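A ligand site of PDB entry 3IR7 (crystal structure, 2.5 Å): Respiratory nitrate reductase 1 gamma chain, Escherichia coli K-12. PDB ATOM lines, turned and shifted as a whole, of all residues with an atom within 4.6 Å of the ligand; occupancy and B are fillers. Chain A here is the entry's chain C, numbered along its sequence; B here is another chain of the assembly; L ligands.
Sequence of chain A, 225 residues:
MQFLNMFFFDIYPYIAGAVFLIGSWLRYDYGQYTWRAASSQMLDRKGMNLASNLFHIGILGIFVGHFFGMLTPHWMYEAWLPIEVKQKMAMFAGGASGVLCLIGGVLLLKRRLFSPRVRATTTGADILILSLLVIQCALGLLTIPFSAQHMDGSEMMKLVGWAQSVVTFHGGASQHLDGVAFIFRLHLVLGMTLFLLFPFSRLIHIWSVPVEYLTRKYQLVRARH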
ATOM      1  N   ALA A  37     -14.982  -2.065   5.562  1.00  0.00           N
ATOM      2  CA  ALA A  37     -15.851  -2.683   6.553  1.00  0.00           C
ATOM      3  C   ALA A  37     -16.351  -1.659   7.549  1.00  0.00           C
ATOM      4  O   ALA A  37     -17.308  -1.901   8.269  1.00  0.00           O
ATOM      5  CB  ALA A  37     -15.110  -3.807   7.269  1.00  0.00           C
ATOM      6  N   SER A  39     -15.000  -0.497  10.399  1.00  0.00           N
ATOM      7  CA  SER A  39     -14.959  -0.948  11.776  1.00  0.00           C
ATOM      8  C   SER A  39     -15.140   0.222  12.715  1.00  0.00           C
ATOM      9  O   SER A  39     -14.661   1.324  12.448  1.00  0.00           O
ATOM     10  CB  SER A  39     -13.637  -1.626  12.082  1.00  0.00           C
ATOM     11  OG  SER A  39     -13.530  -1.865  13.486  1.00  0.00           O
ATOM     12  N   SER A  40     -15.812  -0.030  13.835  1.00  0.00           N
ATOM     13  CA  SER A  40     -16.072   0.984  14.852  1.00  0.00           C
ATOM     14  C   SER A  40     -15.548   0.466  16.179  1.00  0.00           C
ATOM     15  O   SER A  40     -15.674   1.114  17.216  1.00  0.00           O
ATOM     16  CB  SER A  40     -17.582   1.238  14.978  1.00  0.00           C
ATOM     17  OG  SER A  40     -18.248   0.077  15.502  1.00  0.00           O
ATOM     18  N   GLN A  41     -14.938  -0.715  16.132  1.00  0.00           N
ATOM     19  CA  GLN A  41     -14.419  -1.363  17.334  1.00  0.00           C
ATOM     20  C   GLN A  41     -13.498  -0.500  18.190  1.00  0.00           C
ATOM     21  O   GLN A  41     -13.661  -0.429  19.407  1.00  0.00           O
ATOM     22  CB  GLN A  41     -13.705  -2.658  16.947  1.00  0.00           C
ATOM     23  CG  GLN A  41     -13.645  -3.697  18.050  1.00  0.00           C
ATOM     24  CD  GLN A  41     -12.683  -4.831  17.714  1.00  0.00           C
ATOM     25  OE1 GLN A  41     -12.415  -5.116  16.548  1.00  0.00           O
ATOM     26  NE2 GLN A  41     -12.164  -5.481  18.751  1.00  0.00           N
ATOM     27  N   MET A  48     -18.233  -5.588  21.867  1.00  0.00           N
ATOM     28  CA  MET A  48     -18.085  -5.907  20.444  1.00  0.00           C
ATOM     29  C   MET A  48     -17.670  -7.335  20.148  1.00  0.00           C
ATOM     30  O   MET A  48     -18.106  -7.928  19.156  1.00  0.00           O
ATOM     31  CB  MET A  48     -17.097  -4.944  19.777  1.00  0.00           C
ATOM     32  CG  MET A  48     -17.761  -3.726  19.205  1.00  0.00           C
ATOM     33  SD  MET A  48     -19.085  -4.190  18.077  1.00  0.00           S
ATOM     34  CE  MET A  48     -18.239  -4.101  16.520  1.00  0.00           C
ATOM     35  N   SER A  52     -20.490  -8.959  17.933  1.00  0.00           N
ATOM     36  CA  SER A  52     -20.095  -9.125  16.539  1.00  0.00           C
ATOM     37  C   SER A  52     -19.943 -10.591  16.140  1.00  0.00           C
ATOM     38  O   SER A  52     -20.332 -10.972  15.038  1.00  0.00           O
ATOM     39  CB  SER A  52     -18.794  -8.378  16.249  1.00  0.00           C
ATOM     40  OG  SER A  52     -18.515  -8.402  14.858  1.00  0.00           O
ATOM     41  N   PHE A  55     -23.448 -12.179  15.943  1.00  0.00           N
ATOM     42  CA  PHE A  55     -24.095 -11.745  14.712  1.00  0.00           C
ATOM     43  C   PHE A  55     -23.484 -12.382  13.478  1.00  0.00           C
ATOM     44  O   PHE A  55     -24.208 -13.001  12.692  1.00  0.00           O
ATOM     45  CB  PHE A  55     -24.049 -10.212  14.605  1.00  0.00           C
ATOM     46  CG  PHE A  55     -24.637  -9.672  13.331  1.00  0.00           C
ATOM     47  CD1 PHE A  55     -23.829  -9.393  12.245  1.00  0.00           C
ATOM     48  CD2 PHE A  55     -26.008  -9.501  13.205  1.00  0.00           C
ATOM     49  CE1 PHE A  55     -24.381  -8.944  11.042  1.00  0.00           C
ATOM     50  CE2 PHE A  55     -26.570  -9.059  12.015  1.00  0.00           C
ATOM     51  CZ  PHE A  55     -25.757  -8.785  10.922  1.00  0.00           C
ATOM     52  N   HIS A  56     -22.180 -12.267  13.309  1.00  0.00           N
ATOM     53  CA  HIS A  56     -21.549 -12.821  12.116  1.00  0.00           C
ATOM     54  C   HIS A  56     -21.563 -14.331  11.993  1.00  0.00           C
ATOM     55  O   HIS A  56     -21.752 -14.872  10.902  1.00  0.00           O
ATOM     56  CB  HIS A  56     -20.103 -12.297  11.952  1.00  0.00           C
ATOM     57  CG  HIS A  56     -20.029 -10.917  11.355  1.00  0.00           C
ATOM     58  ND1 HIS A  56     -19.936  -9.785  12.136  1.00  0.00           N
ATOM     59  CD2 HIS A  56     -20.119 -10.496  10.076  1.00  0.00           C
ATOM     60  CE1 HIS A  56     -19.986  -8.716  11.355  1.00  0.00           C
ATOM     61  NE2 HIS A  56     -20.101  -9.119  10.097  1.00  0.00           N
ATOM     62  N   ILE A  59     -25.391 -15.099  11.200  1.00  0.00           N
ATOM     63  CA  ILE A  59     -25.757 -14.640   9.857  1.00  0.00           C
ATOM     64  C   ILE A  59     -25.118 -15.497   8.763  1.00  0.00           C
ATOM     65  O   ILE A  59     -25.692 -15.682   7.692  1.00  0.00           O
ATOM     66  CB  ILE A  59     -25.337 -13.171   9.622  1.00  0.00           C
ATOM     67  CG1 ILE A  59     -25.988 -12.633   8.347  1.00  0.00           C
ATOM     68  CG2 ILE A  59     -23.832 -13.076   9.454  1.00  0.00           C
ATOM     69  CD1 ILE A  59     -27.450 -12.276   8.493  1.00  0.00           C
ATOM     70  N   LEU A  60     -23.911 -16.003   9.027  1.00  0.00           N
ATOM     71  CA  LEU A  60     -23.235 -16.839   8.040  1.00  0.00           C
ATOM     72  C   LEU A  60     -23.844 -18.235   8.038  1.00  0.00           C
ATOM     73  O   LEU A  60     -23.826 -18.926   7.011  1.00  0.00           O
ATOM     74  CB  LEU A  60     -21.733 -16.912   8.331  1.00  0.00           C
ATOM     75  CG  LEU A  60     -20.929 -15.665   7.929  1.00  0.00           C
ATOM     76  CD1 LEU A  60     -19.491 -15.775   8.408  1.00  0.00           C
ATOM     77  CD2 LEU A  60     -20.969 -15.487   6.417  1.00  0.00           C
ATOM     78  N   LEU A 108     -25.634  -5.172  18.732  1.00  0.00           N
ATOM     79  CA  LEU A 108     -24.946  -4.237  17.873  1.00  0.00           C
ATOM     80  C   LEU A 108     -25.757  -2.965  17.678  1.00  0.00           C
ATOM     81  O   LEU A 108     -25.216  -1.864  17.706  1.00  0.00           O
ATOM     82  CB  LEU A 108     -24.651  -4.889  16.527  1.00  0.00           C
ATOM     83  CG  LEU A 108     -23.571  -5.969  16.572  1.00  0.00           C
ATOM     84  CD1 LEU A 108     -23.581  -6.784  15.274  1.00  0.00           C
ATOM     85  CD2 LEU A 108     -22.215  -5.315  16.801  1.00  0.00           C
ATOM     86  N   ARG A 111     -25.819  -0.747  20.726  1.00  0.00           N
ATOM     87  CA  ARG A 111     -24.540  -0.066  20.813  1.00  0.00           C
ATOM     88  C   ARG A 111     -24.457   1.092  19.815  1.00  0.00           C
ATOM     89  O   ARG A 111     -24.090   2.210  20.183  1.00  0.00           O
ATOM     90  CB  ARG A 111     -23.410  -1.071  20.551  1.00  0.00           C
ATOM     91  CG  ARG A 111     -22.014  -0.488  20.424  1.00  0.00           C
ATOM     92  CD  ARG A 111     -20.979  -1.599  20.431  1.00  0.00           C
ATOM     93  NE  ARG A 111     -19.674  -1.140  19.975  1.00  0.00           N
ATOM     94  CZ  ARG A 111     -19.423  -0.752  18.734  1.00  0.00           C
ATOM     95  NH1 ARG A 111     -18.202  -0.350  18.398  1.00  0.00           N
ATOM     96  NH2 ARG A 111     -20.391  -0.748  17.818  1.00  0.00           N
ATOM     97  N   ARG A 112     -24.806   0.825  18.553  1.00  0.00           N
ATOM     98  CA  ARG A 112     -24.751   1.858  17.521  1.00  0.00           C
ATOM     99  C   ARG A 112     -25.627   3.063  17.855  1.00  0.00           C
ATOM    100  O   ARG A 112     -25.246   4.198  17.580  1.00  0.00           O
ATOM    101  CB  ARG A 112     -25.162   1.269  16.167  1.00  0.00           C
ATOM    102  CG  ARG A 112     -25.159   2.269  15.024  1.00  0.00           C
ATOM    103  CD  ARG A 112     -25.074   1.560  13.680  1.00  0.00           C
ATOM    104  NE  ARG A 112     -23.825   0.810  13.580  1.00  0.00           N
ATOM    105  CZ  ARG A 112     -22.632   1.383  13.499  1.00  0.00           C
ATOM    106  NH1 ARG A 112     -22.517   2.700  13.502  1.00  0.00           N
ATOM    107  NH2 ARG A 112     -21.533   0.636  13.445  1.00  0.00           N
ATOM    108  N   ASP A 126     -25.777   3.110   8.053  1.00  0.00           N
ATOM    109  CA  ASP A 126     -25.373   2.073   9.005  1.00  0.00           C
ATOM    110  C   ASP A 126     -26.499   1.716   9.962  1.00  0.00           C
ATOM    111  O   ASP A 126     -26.579   0.590  10.440  1.00  0.00           O
ATOM    112  CB  ASP A 126     -24.140   2.502   9.800  1.00  0.00           C
ATOM    113  CG  ASP A 126     -22.962   2.850   8.913  1.00  0.00           C
ATOM    114  OD1 ASP A 126     -22.668   2.076   7.981  1.00  0.00           O
ATOM    115  OD2 ASP A 126     -22.330   3.895   9.167  1.00  0.00           O
ATOM    116  N   ILE A 129     -29.381  -0.102   7.529  1.00  0.00           N
ATOM    117  CA  ILE A 129     -29.057  -1.451   7.101  1.00  0.00           C
ATOM    118  C   ILE A 129     -29.058  -2.442   8.267  1.00  0.00           C
ATOM    119  O   ILE A 129     -29.518  -3.583   8.115  1.00  0.00           O
ATOM    120  CB  ILE A 129     -27.698  -1.484   6.360  1.00  0.00           C
ATOM    121  CG1 ILE A 129     -27.765  -2.468   5.192  1.00  0.00           C
ATOM    122  CG2 ILE A 129     -26.578  -1.878   7.295  1.00  0.00           C
ATOM    123  CD1 ILE A 129     -28.712  -2.038   4.088  1.00  0.00           C
ATOM    124  N   LEU A 130     -28.552  -2.013   9.419  1.00  0.00           N
ATOM    125  CA  LEU A 130     -28.507  -2.865  10.608  1.00  0.00           C
ATOM    126  C   LEU A 130     -29.907  -3.075  11.191  1.00  0.00           C
ATOM    127  O   LEU A 130     -30.198  -4.130  11.767  1.00  0.00           O
ATOM    128  CB  LEU A 130     -27.617  -2.251  11.680  1.00  0.00           C
ATOM    129  CG  LEU A 130     -27.642  -3.053  12.967  1.00  0.00           C
ATOM    130  CD1 LEU A 130     -26.904  -4.362  12.747  1.00  0.00           C
ATOM    131  CD2 LEU A 130     -27.002  -2.263  14.095  1.00  0.00           C
ATOM    132  N   LEU A 133     -31.764  -5.581   8.961  1.00  0.00           N
ATOM    133  CA  LEU A 133     -31.245  -6.943   9.124  1.00  0.00           C
ATOM    134  C   LEU A 133     -31.801  -7.562  10.405  1.00  0.00           C
ATOM    135  O   LEU A 133     -32.138  -8.752  10.427  1.00  0.00           O
ATOM    136  CB  LEU A 133     -29.721  -6.938   9.169  1.00  0.00           C
ATOM    137  CG  LEU A 133     -28.961  -6.816   7.849  1.00  0.00           C
ATOM    138  CD1 LEU A 133     -27.522  -6.419   8.142  1.00  0.00           C
ATOM    139  CD2 LEU A 133     -28.995  -8.141   7.086  1.00  0.00           C
ATOM    140  N   ARG A 202     -22.688  -0.437   3.808  1.00  0.00           N
ATOM    141  CA  ARG A 202     -21.473  -1.117   4.208  1.00  0.00           C
ATOM    142  C   ARG A 202     -21.447  -2.596   3.799  1.00  0.00           C
ATOM    143  O   ARG A 202     -20.396  -3.243   3.867  1.00  0.00           O
ATOM    144  CB  ARG A 202     -21.324  -1.033   5.731  1.00  0.00           C
ATOM    145  CG  ARG A 202     -22.367  -1.829   6.499  1.00  0.00           C
ATOM    146  CD  ARG A 202     -22.385  -1.444   7.968  1.00  0.00           C
ATOM    147  NE  ARG A 202     -21.071  -1.605   8.561  1.00  0.00           N
ATOM    148  CZ  ARG A 202     -20.702  -1.057   9.718  1.00  0.00           C
ATOM    149  NH1 ARG A 202     -21.547  -0.316  10.413  1.00  0.00           N
ATOM    150  NH2 ARG A 202     -19.474  -1.266  10.173  1.00  0.00           N
ATOM    151  N   LEU A 203     -22.592  -3.132   3.360  1.00  0.00           N
ATOM    152  CA  LEU A 203     -22.660  -4.540   2.977  1.00  0.00           C
ATOM    153  C   LEU A 203     -21.655  -4.959   1.913  1.00  0.00           C
ATOM    154  O   LEU A 203     -21.396  -6.154   1.741  1.00  0.00           O
ATOM    155  CB  LEU A 203     -24.069  -4.908   2.505  1.00  0.00           C
ATOM    156  CG  LEU A 203     -25.164  -4.731   3.571  1.00  0.00           C
ATOM    157  CD1 LEU A 203     -26.443  -5.370   3.051  1.00  0.00           C
ATOM    158  CD2 LEU A 203     -24.761  -5.371   4.881  1.00  0.00           C
ATOM    159  N   HIS A 205     -18.735  -5.020   2.085  1.00  0.00           N
ATOM    160  CA  HIS A 205     -17.593  -5.725   2.674  1.00  0.00           C
ATOM    161  C   HIS A 205     -17.717  -7.214   2.418  1.00  0.00           C
ATOM    162  O   HIS A 205     -16.711  -7.901   2.246  1.00  0.00           O
ATOM    163  CB  HIS A 205     -17.410  -5.423   4.186  1.00  0.00           C
ATOM    164  CG  HIS A 205     -18.446  -6.027   5.094  1.00  0.00           C
ATOM    165  ND1 HIS A 205     -19.774  -5.679   5.047  1.00  0.00           N
ATOM    166  CD2 HIS A 205     -18.324  -6.880   6.157  1.00  0.00           C
ATOM    167  CE1 HIS A 205     -20.425  -6.269   6.033  1.00  0.00           C
ATOM    168  NE2 HIS A 205     -19.562  -6.997   6.722  1.00  0.00           N
ATOM    169  N   ILE A 206     -18.963  -7.688   2.355  1.00  0.00           N
ATOM    170  CA  ILE A 206     -19.230  -9.107   2.119  1.00  0.00           C
ATOM    171  C   ILE A 206     -18.515  -9.588   0.867  1.00  0.00           C
ATOM    172  O   ILE A 206     -17.970 -10.687   0.844  1.00  0.00           O
ATOM    173  CB  ILE A 206     -20.743  -9.380   1.984  1.00  0.00           C
ATOM    174  CG1 ILE A 206     -21.465  -8.983   3.260  1.00  0.00           C
ATOM    175  CG2 ILE A 206     -20.986 -10.859   1.722  1.00  0.00           C
ATOM    176  CD1 ILE A 206     -22.968  -8.968   3.105  1.00  0.00           C
ATOM    177  N   VAL A 209     -14.729 -10.855   1.452  1.00  0.00           N
ATOM    178  CA  VAL A 209     -14.321 -11.924   2.371  1.00  0.00           C
ATOM    179  C   VAL A 209     -12.975 -12.456   1.844  1.00  0.00           C
ATOM    180  O   VAL A 209     -12.907 -13.047   0.771  1.00  0.00           O
ATOM    181  CB  VAL A 209     -15.412 -13.035   2.439  1.00  0.00           C
ATOM    182  CG1 VAL A 209     -15.742 -13.553   1.053  1.00  0.00           C
ATOM    183  CG2 VAL A 209     -14.950 -14.159   3.350  1.00  0.00           C
ATOM    184  N   PRO A 210     -11.894 -12.241   2.608  1.00  0.00           N
ATOM    185  CA  PRO A 210     -10.507 -12.638   2.311  1.00  0.00           C
ATOM    186  C   PRO A 210     -10.134 -14.114   2.255  1.00  0.00           C
ATOM    187  O   PRO A 210      -9.286 -14.568   3.026  1.00  0.00           O
ATOM    188  CB  PRO A 210      -9.721 -11.898   3.393  1.00  0.00           C
ATOM    189  CG  PRO A 210     -10.627 -12.033   4.564  1.00  0.00           C
ATOM    190  CD  PRO A 210     -11.995 -11.711   3.977  1.00  0.00           C
ATOM    191  N   ILE B  88     -11.439 -12.082  12.803  1.00  0.00           N
ATOM    192  CA  ILE B  88     -11.875 -10.943  12.012  1.00  0.00           C
ATOM    193  C   ILE B  88     -13.184 -10.220  12.367  1.00  0.00           C
ATOM    194  O   ILE B  88     -13.303  -9.020  12.103  1.00  0.00           O
ATOM    195  CB  ILE B  88     -11.920 -11.338  10.519  1.00  0.00           C
ATOM    196  CG1 ILE B  88     -11.839 -10.092   9.640  1.00  0.00           C
ATOM    197  CG2 ILE B  88     -13.187 -12.135  10.240  1.00  0.00           C
ATOM    198  CD1 ILE B  88     -11.395 -10.370   8.216  1.00  0.00           C
ATOM    199  N   PHE B  89     -14.147 -10.917  12.956  1.00  0.00           N
ATOM    200  CA  PHE B  89     -15.395 -10.236  13.284  1.00  0.00           C
ATOM    201  C   PHE B  89     -15.167  -9.230  14.382  1.00  0.00           C
ATOM    202  O   PHE B  89     -15.835  -8.195  14.432  1.00  0.00           O
ATOM    203  CB  PHE B  89     -16.468 -11.259  13.668  1.00  0.00           C
ATOM    204  CG  PHE B  89     -16.713 -12.289  12.615  1.00  0.00           C
ATOM    205  CD1 PHE B  89     -16.921 -11.899  11.289  1.00  0.00           C
ATOM    206  CD2 PHE B  89     -16.711 -13.637  12.924  1.00  0.00           C
ATOM    207  CE1 PHE B  89     -17.114 -12.859  10.281  1.00  0.00           C
ATOM    208  CE2 PHE B  89     -16.898 -14.610  11.929  1.00  0.00           C
ATOM    209  CZ  PHE B  89     -17.097 -14.214  10.605  1.00  0.00           C
ATOM    210  N   TRP B 220     -10.006  -4.401   7.556  1.00  0.00           N
ATOM    211  CA  TRP B 220     -10.112  -5.612   8.379  1.00  0.00           C
ATOM    212  C   TRP B 220      -9.407  -5.397   9.729  1.00  0.00           C
ATOM    213  O   TRP B 220      -9.513  -6.217  10.638  1.00  0.00           O
ATOM    214  CB  TRP B 220      -9.461  -6.808   7.660  1.00  0.00           C
ATOM    215  CG  TRP B 220     -10.124  -7.196   6.344  1.00  0.00           C
ATOM    216  CD1 TRP B 220      -9.493  -7.497   5.177  1.00  0.00           C
ATOM    217  CD2 TRP B 220     -11.524  -7.347   6.095  1.00  0.00           C
ATOM    218  NE1 TRP B 220     -10.413  -7.823   4.210  1.00  0.00           N
ATOM    219  CE2 TRP B 220     -11.672  -7.744   4.740  1.00  0.00           C
ATOM    220  CE3 TRP B 220     -12.674  -7.199   6.877  1.00  0.00           C
ATOM    221  CZ2 TRP B 220     -12.912  -7.985   4.161  1.00  0.00           C
ATOM    222  CZ3 TRP B 220     -13.917  -7.433   6.291  1.00  0.00           C
ATOM    223  CH2 TRP B 220     -14.022  -7.825   4.950  1.00  0.00           C
ATOM    224  N   ARG B 221      -8.704  -4.268   9.838  1.00  0.00           N
ATOM    225  CA  ARG B 221      -7.971  -3.877  11.049  1.00  0.00           C
ATOM    226  C   ARG B 221      -7.250  -4.968  11.867  1.00  0.00           C
ATOM    227  O   ARG B 221      -7.340  -4.985  13.096  1.00  0.00           O
ATOM    228  CB  ARG B 221      -8.904  -3.078  11.962  1.00  0.00           C
ATOM    229  CG  ARG B 221     -10.263  -3.718  12.223  1.00  0.00           C
ATOM    230  CD  ARG B 221     -10.296  -4.466  13.538  1.00  0.00           C
ATOM    231  NE  ARG B 221     -11.615  -4.999  13.838  1.00  0.00           N
ATOM    232  CZ  ARG B 221     -12.160  -6.063  13.240  1.00  0.00           C
ATOM    233  NH1 ARG B 221     -11.483  -6.724  12.305  1.00  0.00           N
ATOM    234  NH2 ARG B 221     -13.369  -6.466  13.585  1.00  0.00           N
HETATM  235  C1  LIG L   1     -19.542  -5.308  10.280  1.00  0.00           C
HETATM  236  C2  LIG L   1     -16.431  -8.615   8.617  1.00  0.00           C
HETATM  237  C3  LIG L   1     -20.170 -10.886   6.501  1.00  0.00           C
HETATM  238  C4  LIG L   1     -23.258  -7.570   8.146  1.00  0.00           C
HETATM  239  C5  LIG L   1     -18.361  -5.988  10.029  1.00  0.00           C
HETATM  240  C6  LIG L   1     -17.012  -5.637  10.485  1.00  0.00           C
HETATM  241  C7  LIG L   1     -16.160  -6.548  10.035  1.00  0.00           C
HETATM  242  C8  LIG L   1     -16.954  -7.507   9.262  1.00  0.00           C
HETATM  243  C9  LIG L   1     -14.599  -6.653  10.221  1.00  0.00           C
HETATM  244  C10 LIG L   1     -16.699  -4.384  11.352  1.00  0.00           C
HETATM  245  C11 LIG L   1     -16.765  -4.736  12.893  1.00  0.00           C
HETATM  246  C12 LIG L   1     -16.060  -3.779  13.856  1.00  0.00           C
HETATM  247  O1  LIG L   1     -14.876  -4.069  14.209  1.00  0.00           O
HETATM  248  O2  LIG L   1     -16.713  -2.745  14.195  1.00  0.00           O
HETATM  249  C13 LIG L   1     -17.186  -9.539   7.889  1.00  0.00           C
HETATM  250  C14 LIG L   1     -16.640 -10.716   7.195  1.00  0.00           C
HETATM  251  C15 LIG L   1     -17.684 -11.347   6.598  1.00  0.00           C
HETATM  252  C16 LIG L   1     -18.894 -10.577   6.920  1.00  0.00           C
HETATM  253  C17 LIG L   1     -15.119 -11.080   7.207  1.00  0.00           C
HETATM  254  C18 LIG L   1     -17.685 -12.661   5.711  1.00  0.00           C
HETATM  255  C19 LIG L   1     -17.248 -13.898   6.124  1.00  0.00           C
HETATM  256  C20 LIG L   1     -21.350 -10.205   6.752  1.00  0.00           C
HETATM  257  C21 LIG L   1     -22.695 -10.579   6.287  1.00  0.00           C
HETATM  258  C22 LIG L   1     -23.549  -9.652   6.752  1.00  0.00           C
HETATM  259  C23 LIG L   1     -22.753  -8.674   7.514  1.00  0.00           C
HETATM  260  C24 LIG L   1     -23.002 -11.854   5.411  1.00  0.00           C
HETATM  261  C25 LIG L   1     -25.104  -9.508   6.586  1.00  0.00           C
HETATM  262  C26 LIG L   1     -25.625  -9.315   5.340  1.00  0.00           C
HETATM  263  C27 LIG L   1     -22.519  -6.658   8.871  1.00  0.00           C
HETATM  264  C28 LIG L   1     -23.092  -5.474   9.555  1.00  0.00           C
HETATM  265  C29 LIG L   1     -22.049  -4.860  10.150  1.00  0.00           C
HETATM  266  C30 LIG L   1     -20.824  -5.637   9.843  1.00  0.00           C
HETATM  267  C31 LIG L   1     -24.600  -5.066   9.565  1.00  0.00           C
HETATM  268  C32 LIG L   1     -21.991  -3.576  11.054  1.00  0.00           C
HETATM  269  C33 LIG L   1     -22.472  -3.773  12.550  1.00  0.00           C
HETATM  270  C34 LIG L   1     -22.717  -2.458  13.305  1.00  0.00           C
HETATM  271  O3  LIG L   1     -21.881  -2.158  14.230  1.00  0.00           O
HETATM  272  O4  LIG L   1     -23.750  -1.779  12.935  1.00  0.00           O
HETATM  273  N1  LIG L   1     -18.294  -7.144   9.279  1.00  0.00           N
HETATM  274  N2  LIG L   1     -18.561  -9.482   7.698  1.00  0.00           N
HETATM  275  N3  LIG L   1     -21.409  -9.044   7.503  1.00  0.00           N
HETATM  276  N4  LIG L   1     -21.145  -6.717   9.076  1.00  0.00           N
HETATM  277 FE1  LIG L   1     -19.830  -8.070   8.412  1.00  0.00          FE
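The guanidinium group of Arg 221 of chain B is in salt-bridge range of an oxygen (O1) of the ligand (2.9 Å).
A ring nitrogen (NE2) of His 205 is bound to an iron atom (FE1) of the ligand, at 2.0 Å.
An oxygen (O1) of the ligand is in hydrogen-bond range of the side-chain hydroxyl (OG) of Ser 39 (2.7 Å).
The backbone NH (N) of Gln 41 lies within hydrogen-bond range of an oxygen (O2) of the ligand, at 3.3 Å.
OG of Ser 40 sits at hydrogen-bond distance from O2 of the ligand, 3.5 Å away.
The guanidinium group (NH1) of Arg 202 is in salt-bridge range of an oxygen (O4) of the ligand (3.7 Å).
NE2 of His 56 is bound to FE1 of the ligand, 2.0 Å away.
N of Ser 40 sits at hydrogen-bond distance from O2 of the ligand.
NE of Arg 112 is in salt-bridge range of O4 of the ligand (2.7 Å).
NH2 of Arg 221 of chain B is in hydrogen-bond range of O of Phe 89 of chain B (3.1 Å).
The guanidinium group of Arg 221 of chain B sits at hydrogen-bond distance from the side-chain amide oxygen of Gln 41 (2.8 Å).
SD of Met 48 lies close to NE of Arg 111 (3.6 Å).
A ring nitrogen (ND1) of His 56 lies within hydrogen-bond range of the backbone carbonyl oxygen (O) of Ser 52, at 3.2 Å.
NH1 of Arg 202 is in salt-bridge range of OD1 of Asp 126 (3.6 Å).
The backbone carbonyl oxygen (O) of Ala 37 is in hydrogen-bond range of the guanidinium group (NH2) of Arg 202 (3.0 Å).
NH1 of Arg 111 is in hydrogen-bond range of OG of Ser 40 (2.9 Å).
ND1 of His 205 is in hydrogen-bond range of O of Arg 202 (2.8 Å).
Met 48 touches the ligand.
CE1 of Phe 55 touches C4 of the ligand, at 3.4 Å.
Ile 59 touches the ligand.
Leu 60 touches the ligand.
Leu 130 touches the ligand.
Leu 133 touches the ligand (CD1 to C31, 3.5 Å).
Ile 206 touches the ligand.
Val 209 touches the ligand (CG2 to C19, 3.6 Å).
Ile 88 of chain B touches the ligand (O to C9, 3.3 Å).
Phe 89 of chain B touches the ligand.
CZ3 of Trp 220 of chain B touches C2 of the ligand, 3.6 Å away.
Hydrophobic or aromatic side chains that line the ligand: Met 48, Phe 55, His 56, Ile 59, Leu 60, Leu 130, Leu 133, His 205, Ile 206, Val 209, Ile 88 of chain B, Phe 89 of chain B and Trp 220 of chain B.
The nearest printed residue that does not touch the ligand is Ala 37 (4.01 Å).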
